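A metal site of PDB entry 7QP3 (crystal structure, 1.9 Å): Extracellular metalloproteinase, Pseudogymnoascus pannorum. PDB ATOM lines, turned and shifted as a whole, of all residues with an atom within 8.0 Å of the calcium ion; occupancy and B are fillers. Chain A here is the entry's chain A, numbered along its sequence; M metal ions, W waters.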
ATOM      1  N   PHE A 113     -13.523   1.747 -13.739  1.00  0.00           N
ATOM      2  CA  PHE A 113     -14.713   1.589 -12.897  1.00  0.00           C
ATOM      3  C   PHE A 113     -14.403   0.515 -11.874  1.00  0.00           C
ATOM      4  O   PHE A 113     -14.802  -0.641 -11.975  1.00  0.00           O
ATOM      5  CB  PHE A 113     -15.960   1.241 -13.704  1.00  0.00           C
ATOM      6  CG  PHE A 113     -17.205   1.223 -12.865  1.00  0.00           C
ATOM      7  CD1 PHE A 113     -17.584   2.345 -12.141  1.00  0.00           C
ATOM      8  CD2 PHE A 113     -17.989   0.066 -12.788  1.00  0.00           C
ATOM      9  CE1 PHE A 113     -18.723   2.324 -11.354  1.00  0.00           C
ATOM     10  CE2 PHE A 113     -19.103   0.053 -12.026  1.00  0.00           C
ATOM     11  CZ  PHE A 113     -19.487   1.189 -11.319  1.00  0.00           C
ATOM     12  N   ASN A 114     -13.656   0.934 -10.862  1.00  0.00           N
ATOM     13  CA  ASN A 114     -13.088   0.027  -9.895  1.00  0.00           C
ATOM     14  C   ASN A 114     -13.689   0.282  -8.511  1.00  0.00           C
ATOM     15  O   ASN A 114     -14.723   0.938  -8.373  1.00  0.00           O
ATOM     16  CB  ASN A 114     -11.565   0.209  -9.876  1.00  0.00           C
ATOM     17  CG  ASN A 114     -11.162   1.621  -9.601  1.00  0.00           C
ATOM     18  OD1 ASN A 114     -11.950   2.436  -9.118  1.00  0.00           O
ATOM     19  ND2 ASN A 114      -9.922   1.949  -9.938  1.00  0.00           N
ATOM     20  N   GLU A 115     -13.032  -0.233  -7.484  1.00  0.00           N
ATOM     21  CA  GLU A 115     -13.575  -0.180  -6.127  1.00  0.00           C
ATOM     22  C   GLU A 115     -13.833   1.252  -5.676  1.00  0.00           C
ATOM     23  O   GLU A 115     -14.947   1.589  -5.256  1.00  0.00           O
ATOM     24  CB  GLU A 115     -12.595  -0.897  -5.196  1.00  0.00           C
ATOM     25  CG  GLU A 115     -12.424  -2.377  -5.516  1.00  0.00           C
ATOM     26  CD  GLU A 115     -11.339  -2.679  -6.544  1.00  0.00           C
ATOM     27  OE1 GLU A 115     -10.758  -1.771  -7.164  1.00  0.00           O
ATOM     28  OE2 GLU A 115     -11.051  -3.869  -6.737  1.00  0.00           O
ATOM     29  N   ALA A 116     -12.832   2.118  -5.754  1.00  0.00           N
ATOM     30  CA  ALA A 116     -12.991   3.493  -5.309  1.00  0.00           C
ATOM     31  C   ALA A 116     -13.931   4.297  -6.203  1.00  0.00           C
ATOM     32  O   ALA A 116     -14.471   5.305  -5.751  1.00  0.00           O
ATOM     33  CB  ALA A 116     -11.629   4.185  -5.258  1.00  0.00           C
ATOM     34  N   ALA A 117     -14.167   3.872  -7.448  1.00  0.00           N
ATOM     35  CA  ALA A 117     -15.073   4.597  -8.334  1.00  0.00           C
ATOM     36  C   ALA A 117     -16.554   4.321  -8.061  1.00  0.00           C
ATOM     37  O   ALA A 117     -17.415   5.024  -8.605  1.00  0.00           O
ATOM     38  CB  ALA A 117     -14.764   4.258  -9.786  1.00  0.00           C
ATOM     39  N   GLY A 118     -16.831   3.317  -7.240  1.00  0.00           N
ATOM     40  CA  GLY A 118     -18.187   2.962  -6.885  1.00  0.00           C
ATOM     41  C   GLY A 118     -18.712   1.726  -7.564  1.00  0.00           C
ATOM     42  O   GLY A 118     -19.903   1.682  -7.851  1.00  0.00           O
ATOM     43  N   ASN A 119     -17.852   0.748  -7.876  1.00  0.00           N
ATOM     44  CA  ASN A 119     -18.283  -0.439  -8.621  1.00  0.00           C
ATOM     45  C   ASN A 119     -19.021  -1.410  -7.699  1.00  0.00           C
ATOM     46  O   ASN A 119     -19.397  -1.046  -6.586  1.00  0.00           O
ATOM     47  CB  ASN A 119     -17.085  -1.048  -9.360  1.00  0.00           C
ATOM     48  CG  ASN A 119     -16.207  -1.952  -8.491  1.00  0.00           C
ATOM     49  OD1 ASN A 119     -16.222  -1.899  -7.270  1.00  0.00           O
ATOM     50  ND2 ASN A 119     -15.398  -2.764  -9.152  1.00  0.00           N
ATOM     51  N   PHE A 120     -19.283  -2.642  -8.189  1.00  0.00           N
ATOM     52  CA  PHE A 120     -20.194  -3.610  -7.557  1.00  0.00           C
ATOM     53  C   PHE A 120     -19.404  -4.845  -7.180  1.00  0.00           C
ATOM     54  O   PHE A 120     -19.120  -5.681  -8.041  1.00  0.00           O
ATOM     55  CB  PHE A 120     -21.349  -3.998  -8.486  1.00  0.00           C
ATOM     56  CG  PHE A 120     -22.211  -2.858  -8.923  1.00  0.00           C
ATOM     57  CD1 PHE A 120     -23.268  -2.415  -8.133  1.00  0.00           C
ATOM     58  CD2 PHE A 120     -21.976  -2.230 -10.141  1.00  0.00           C
ATOM     59  CE1 PHE A 120     -24.061  -1.351  -8.553  1.00  0.00           C
ATOM     60  CE2 PHE A 120     -22.763  -1.178 -10.562  1.00  0.00           C
ATOM     61  CZ  PHE A 120     -23.806  -0.728  -9.758  1.00  0.00           C
ATOM     62  N   GLU A 121     -19.022  -4.958  -5.895  1.00  0.00           N
ATOM     63  CA  GLU A 121     -18.302  -6.125  -5.402  1.00  0.00           C
ATOM     64  C   GLU A 121     -18.585  -6.319  -3.919  1.00  0.00           C
ATOM     65  O   GLU A 121     -18.908  -5.377  -3.203  1.00  0.00           O
ATOM     66  CB  GLU A 121     -16.795  -6.002  -5.555  1.00  0.00           C
ATOM     67  CG  GLU A 121     -16.297  -5.662  -6.973  1.00  0.00           C
ATOM     68  CD  GLU A 121     -14.796  -5.425  -7.003  1.00  0.00           C
ATOM     69  OE1 GLU A 121     -14.206  -5.509  -5.907  1.00  0.00           O
ATOM     70  OE2 GLU A 121     -14.205  -5.202  -8.078  1.00  0.00           O
ATOM     71  N   THR A 122     -18.450  -7.566  -3.486  1.00  0.00           N
ATOM     72  CA  THR A 122     -18.661  -7.896  -2.074  1.00  0.00           C
ATOM     73  C   THR A 122     -17.510  -7.377  -1.219  1.00  0.00           C
ATOM     74  O   THR A 122     -17.723  -6.719  -0.194  1.00  0.00           O
ATOM     75  CB  THR A 122     -18.794  -9.399  -1.935  1.00  0.00           C
ATOM     76  OG1 THR A 122     -19.911  -9.829  -2.707  1.00  0.00           O
ATOM     77  CG2 THR A 122     -18.958  -9.817  -0.510  1.00  0.00           C
ATOM     78  N   ASN A 123     -16.282  -7.664  -1.638  1.00  0.00           N
ATOM     79  CA  ASN A 123     -15.056  -7.374  -0.898  1.00  0.00           C
ATOM     80  C   ASN A 123     -14.173  -6.500  -1.790  1.00  0.00           C
ATOM     81  O   ASN A 123     -13.647  -6.979  -2.799  1.00  0.00           O
ATOM     82  CB  ASN A 123     -14.360  -8.689  -0.512  1.00  0.00           C
ATOM     83  CG  ASN A 123     -13.092  -8.483   0.287  1.00  0.00           C
ATOM     84  OD1 ASN A 123     -12.724  -7.364   0.648  1.00  0.00           O
ATOM     85  ND2 ASN A 123     -12.416  -9.578   0.614  1.00  0.00           N
ATOM     86  N   ASN A 124     -14.025  -5.223  -1.420  1.00  0.00           N
ATOM     87  CA  ASN A 124     -13.132  -4.318  -2.149  1.00  0.00           C
ATOM     88  C   ASN A 124     -11.665  -4.501  -1.803  1.00  0.00           C
ATOM     89  O   ASN A 124     -10.799  -3.893  -2.451  1.00  0.00           O
ATOM     90  CB  ASN A 124     -13.565  -2.872  -1.904  1.00  0.00           C
ATOM     91  CG  ASN A 124     -14.876  -2.562  -2.540  1.00  0.00           C
ATOM     92  OD1 ASN A 124     -15.536  -3.450  -3.062  1.00  0.00           O
ATOM     93  ND2 ASN A 124     -15.262  -1.291  -2.526  1.00  0.00           N
ATOM     94  N   GLY A 128     -10.596   0.799  -1.389  1.00  0.00           N
ATOM     95  CA  GLY A 128     -11.454   1.957  -1.251  1.00  0.00           C
ATOM     96  C   GLY A 128     -12.899   1.629  -1.587  1.00  0.00           C
ATOM     97  O   GLY A 128     -13.266   0.501  -1.902  1.00  0.00           O
ATOM     98  N   GLY A 129     -13.735   2.664  -1.524  1.00  0.00           N
ATOM     99  CA  GLY A 129     -15.167   2.520  -1.774  1.00  0.00           C
ATOM    100  C   GLY A 129     -15.841   1.613  -0.726  1.00  0.00           C
ATOM    101  O   GLY A 129     -15.280   1.271   0.290  1.00  0.00           O
ATOM    102  N   LYS A 130     -17.069   1.214  -1.039  1.00  0.00           N
ATOM    103  CA  LYS A 130     -17.877   0.368  -0.171  1.00  0.00           C
ATOM    104  C   LYS A 130     -18.217  -0.941  -0.854  1.00  0.00           C
ATOM    105  O   LYS A 130     -18.642  -0.947  -2.028  1.00  0.00           O
ATOM    106  CB  LYS A 130     -19.167   1.071   0.205  1.00  0.00           C
ATOM    107  CG  LYS A 130     -18.946   2.429   0.816  1.00  0.00           C
ATOM    108  CD  LYS A 130     -20.228   2.931   1.410  1.00  0.00           C
ATOM    109  CE  LYS A 130     -19.942   4.091   2.357  1.00  0.00           C
ATOM    110  NZ  LYS A 130     -20.444   5.354   1.777  1.00  0.00           N
ATOM    111  N   GLY A 131     -18.057  -2.032  -0.132  1.00  0.00           N
ATOM    112  CA  GLY A 131     -18.360  -3.352  -0.643  1.00  0.00           C
ATOM    113  C   GLY A 131     -19.794  -3.748  -0.354  1.00  0.00           C
ATOM    114  O   GLY A 131     -20.674  -2.891  -0.181  1.00  0.00           O
ATOM    115  N   ASN A 132     -20.004  -5.065  -0.262  1.00  0.00           N
ATOM    116  CA  ASN A 132     -21.309  -5.678  -0.058  1.00  0.00           C
ATOM    117  C   ASN A 132     -22.288  -5.288  -1.148  1.00  0.00           C
ATOM    118  O   ASN A 132     -23.490  -5.239  -0.911  1.00  0.00           O
ATOM    119  CB  ASN A 132     -21.851  -5.331   1.314  1.00  0.00           C
ATOM    120  CG  ASN A 132     -20.957  -5.802   2.392  1.00  0.00           C
ATOM    121  OD1 ASN A 132     -20.535  -6.964   2.394  1.00  0.00           O
ATOM    122  ND2 ASN A 132     -20.614  -4.910   3.315  1.00  0.00           N
ATOM    123  N   ASP A 133     -21.807  -5.057  -2.370  1.00  0.00           N
ATOM    124  CA  ASP A 133     -22.735  -4.640  -3.404  1.00  0.00           C
ATOM    125  C   ASP A 133     -22.426  -5.344  -4.710  1.00  0.00           C
ATOM    126  O   ASP A 133     -22.583  -4.791  -5.807  1.00  0.00           O
ATOM    127  CB  ASP A 133     -22.783  -3.103  -3.525  1.00  0.00           C
ATOM    128  CG  ASP A 133     -21.447  -2.430  -3.930  1.00  0.00           C
ATOM    129  OD1 ASP A 133     -20.397  -3.071  -4.017  1.00  0.00           O
ATOM    130  OD2 ASP A 133     -21.472  -1.186  -4.145  1.00  0.00           O
ATOM    131  N   ALA A 134     -22.082  -6.628  -4.607  1.00  0.00           N
ATOM    132  CA  ALA A 134     -22.024  -7.483  -5.784  1.00  0.00           C
ATOM    133  C   ALA A 134     -23.409  -7.501  -6.424  1.00  0.00           C
ATOM    134  O   ALA A 134     -24.421  -7.428  -5.740  1.00  0.00           O
ATOM    135  CB  ALA A 134     -21.558  -8.881  -5.393  1.00  0.00           C
ATOM    136  N   PRO A 154     -27.113   3.558  -3.933  1.00  0.00           N
ATOM    137  CA  PRO A 154     -25.775   4.114  -3.695  1.00  0.00           C
ATOM    138  C   PRO A 154     -24.757   3.029  -3.368  1.00  0.00           C
ATOM    139  O   PRO A 154     -25.098   1.910  -2.995  1.00  0.00           O
ATOM    140  CB  PRO A 154     -25.982   5.063  -2.514  1.00  0.00           C
ATOM    141  CG  PRO A 154     -27.425   5.478  -2.621  1.00  0.00           C
ATOM    142  CD  PRO A 154     -28.158   4.246  -3.156  1.00  0.00           C
ATOM    143  N   ASP A 155     -23.488   3.391  -3.534  1.00  0.00           N
ATOM    144  CA  ASP A 155     -22.391   2.476  -3.261  1.00  0.00           C
ATOM    145  C   ASP A 155     -22.560   1.853  -1.876  1.00  0.00           C
ATOM    146  O   ASP A 155     -22.956   2.531  -0.923  1.00  0.00           O
ATOM    147  CB  ASP A 155     -21.062   3.220  -3.348  1.00  0.00           C
ATOM    148  CG  ASP A 155     -19.870   2.316  -3.582  1.00  0.00           C
ATOM    149  OD1 ASP A 155     -20.069   1.169  -4.055  1.00  0.00           O
ATOM    150  OD2 ASP A 155     -18.741   2.765  -3.276  1.00  0.00           O
ATOM    151  N   GLY A 156     -22.294   0.565  -1.772  1.00  0.00           N
ATOM    152  CA  GLY A 156     -22.511  -0.160  -0.539  1.00  0.00           C
ATOM    153  C   GLY A 156     -23.794  -0.967  -0.476  1.00  0.00           C
ATOM    154  O   GLY A 156     -23.978  -1.710   0.478  1.00  0.00           O
ATOM    155  N   GLN A 157     -24.696  -0.807  -1.455  1.00  0.00           N
ATOM    156  CA  GLN A 157     -25.883  -1.625  -1.546  1.00  0.00           C
ATOM    157  C   GLN A 157     -25.968  -2.243  -2.935  1.00  0.00           C
ATOM    158  O   GLN A 157     -25.576  -1.599  -3.917  1.00  0.00           O
ATOM    159  CB  GLN A 157     -27.150  -0.806  -1.289  1.00  0.00           C
ATOM    160  CG  GLN A 157     -27.185  -0.117   0.047  1.00  0.00           C
ATOM    161  CD  GLN A 157     -28.107   1.118   0.005  1.00  0.00           C
ATOM    162  OE1 GLN A 157     -27.654   2.263   0.134  1.00  0.00           O
ATOM    163  NE2 GLN A 157     -29.387   0.880  -0.208  1.00  0.00           N
ATOM    164  N   PRO A 158     -26.480  -3.471  -3.057  1.00  0.00           N
ATOM    165  CA  PRO A 158     -26.306  -4.215  -4.307  1.00  0.00           C
ATOM    166  C   PRO A 158     -27.076  -3.621  -5.455  1.00  0.00           C
ATOM    167  O   PRO A 158     -28.229  -3.222  -5.301  1.00  0.00           O
ATOM    168  CB  PRO A 158     -26.845  -5.610  -3.964  1.00  0.00           C
ATOM    169  CG  PRO A 158     -26.870  -5.664  -2.482  1.00  0.00           C
ATOM    170  CD  PRO A 158     -27.083  -4.297  -1.998  1.00  0.00           C
ATOM    171  N   ARG A 193     -23.832   5.125 -10.822  1.00  0.00           N
ATOM    172  CA  ARG A 193     -22.781   5.278  -9.815  1.00  0.00           C
ATOM    173  C   ARG A 193     -21.838   6.424 -10.160  1.00  0.00           C
ATOM    174  O   ARG A 193     -21.571   7.309  -9.322  1.00  0.00           O
ATOM    175  CB  ARG A 193     -22.001   3.965  -9.664  1.00  0.00           C
ATOM    176  CG  ARG A 193     -22.757   2.860  -8.906  1.00  0.00           C
ATOM    177  CD  ARG A 193     -22.782   3.132  -7.393  1.00  0.00           C
ATOM    178  NE  ARG A 193     -23.658   2.213  -6.686  1.00  0.00           N
ATOM    179  CZ  ARG A 193     -23.309   1.007  -6.253  1.00  0.00           C
ATOM    180  NH1 ARG A 193     -22.090   0.524  -6.426  1.00  0.00           N
ATOM    181  NH2 ARG A 193     -24.213   0.249  -5.655  1.00  0.00           N
ATOM    182  N   PRO A 198     -20.474   8.167  -6.458  1.00  0.00           N
ATOM    183  CA  PRO A 198     -21.081   6.873  -6.131  1.00  0.00           C
ATOM    184  C   PRO A 198     -22.111   6.884  -5.000  1.00  0.00           C
ATOM    185  O   PRO A 198     -22.843   5.909  -4.856  1.00  0.00           O
ATOM    186  CB  PRO A 198     -19.860   6.016  -5.754  1.00  0.00           C
ATOM    187  CG  PRO A 198     -18.808   6.980  -5.352  1.00  0.00           C
ATOM    188  CD  PRO A 198     -19.046   8.223  -6.119  1.00  0.00           C
HETATM  189 CA    CA M   1     -19.140  -0.908  -4.276  1.00  0.00          CA
HETATM  190  O   HOH W   1     -17.277   0.585  -4.363  1.00  0.00           O
HETATM  191  O   HOH W   2     -17.350  -2.394  -4.803  1.00  0.00           O
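Water W1 lies within hydrogen-bond range of the backbone carbonyl oxygen (O) of Glu 115 (2.7 Å), the side-chain carboxylate (OD2) of Asp 155 (2.8 Å), the side-chain amide nitrogen (ND2) of Asn 124 (3.3 Å) and the backbone NH (N) of Lys 130 (3.4 Å).
Water W2 lies within hydrogen-bond range of the side-chain amide oxygen of Asn 124, the side-chain amide oxygen of Asn 119 and the backbone NH of Glu 121.
O of Pro 198 sits at hydrogen-bond distance from N of Asp 155 (2.9 Å).
The backbone carbonyl oxygen (O) of Asn 119 sits close to the guanidinium group (NH1) of Arg 193.
The side-chain amide nitrogen (ND2) of Asn 119 sits close to the side-chain carboxylate (OE2) of Glu 121 (2.9 Å).
The guanidinium group (NH1) of Arg 193 sits close to the side-chain carboxylate (OD2) of Asp 133 (2.9 Å).
The backbone NH (N) of Asp 133 lies within hydrogen-bond range of the backbone carbonyl oxygen (O) of Glu 121, at 3.0 Å.
The guanidinium group of Arg 193 lies within hydrogen-bond range of the backbone carbonyl oxygen of Gly 118, at 2.9 Å.
The guanidinium group (NH2) of Arg 193 is in hydrogen-bond range of the backbone carbonyl oxygen (O) of Gln 157 (2.9 Å).
The guanidinium group (NH2) of Arg 193 is in hydrogen-bond range of the backbone carbonyl oxygen (O) of Pro 154 (3.3 Å).
The calcium ion is bound by OD1 of Asp 155 (2.3 Å), O of Lys 130 (2.3 Å), O of Asn 119 (2.3 Å), OD2 of Asp 133 (2.4 Å), water W2 (2.4 Å), water W1 (2.4 Å) and OD1 of Asp 133 (2.5 Å).
Arg 193 touches the calcium ion (NH1 to CA, 3.9 Å).
Of the 26 residues printed, 5 come within 4 Å of the calcium ion.
The nearest printed residue that does not touch the calcium ion is Gly 118 (4.2 Å).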
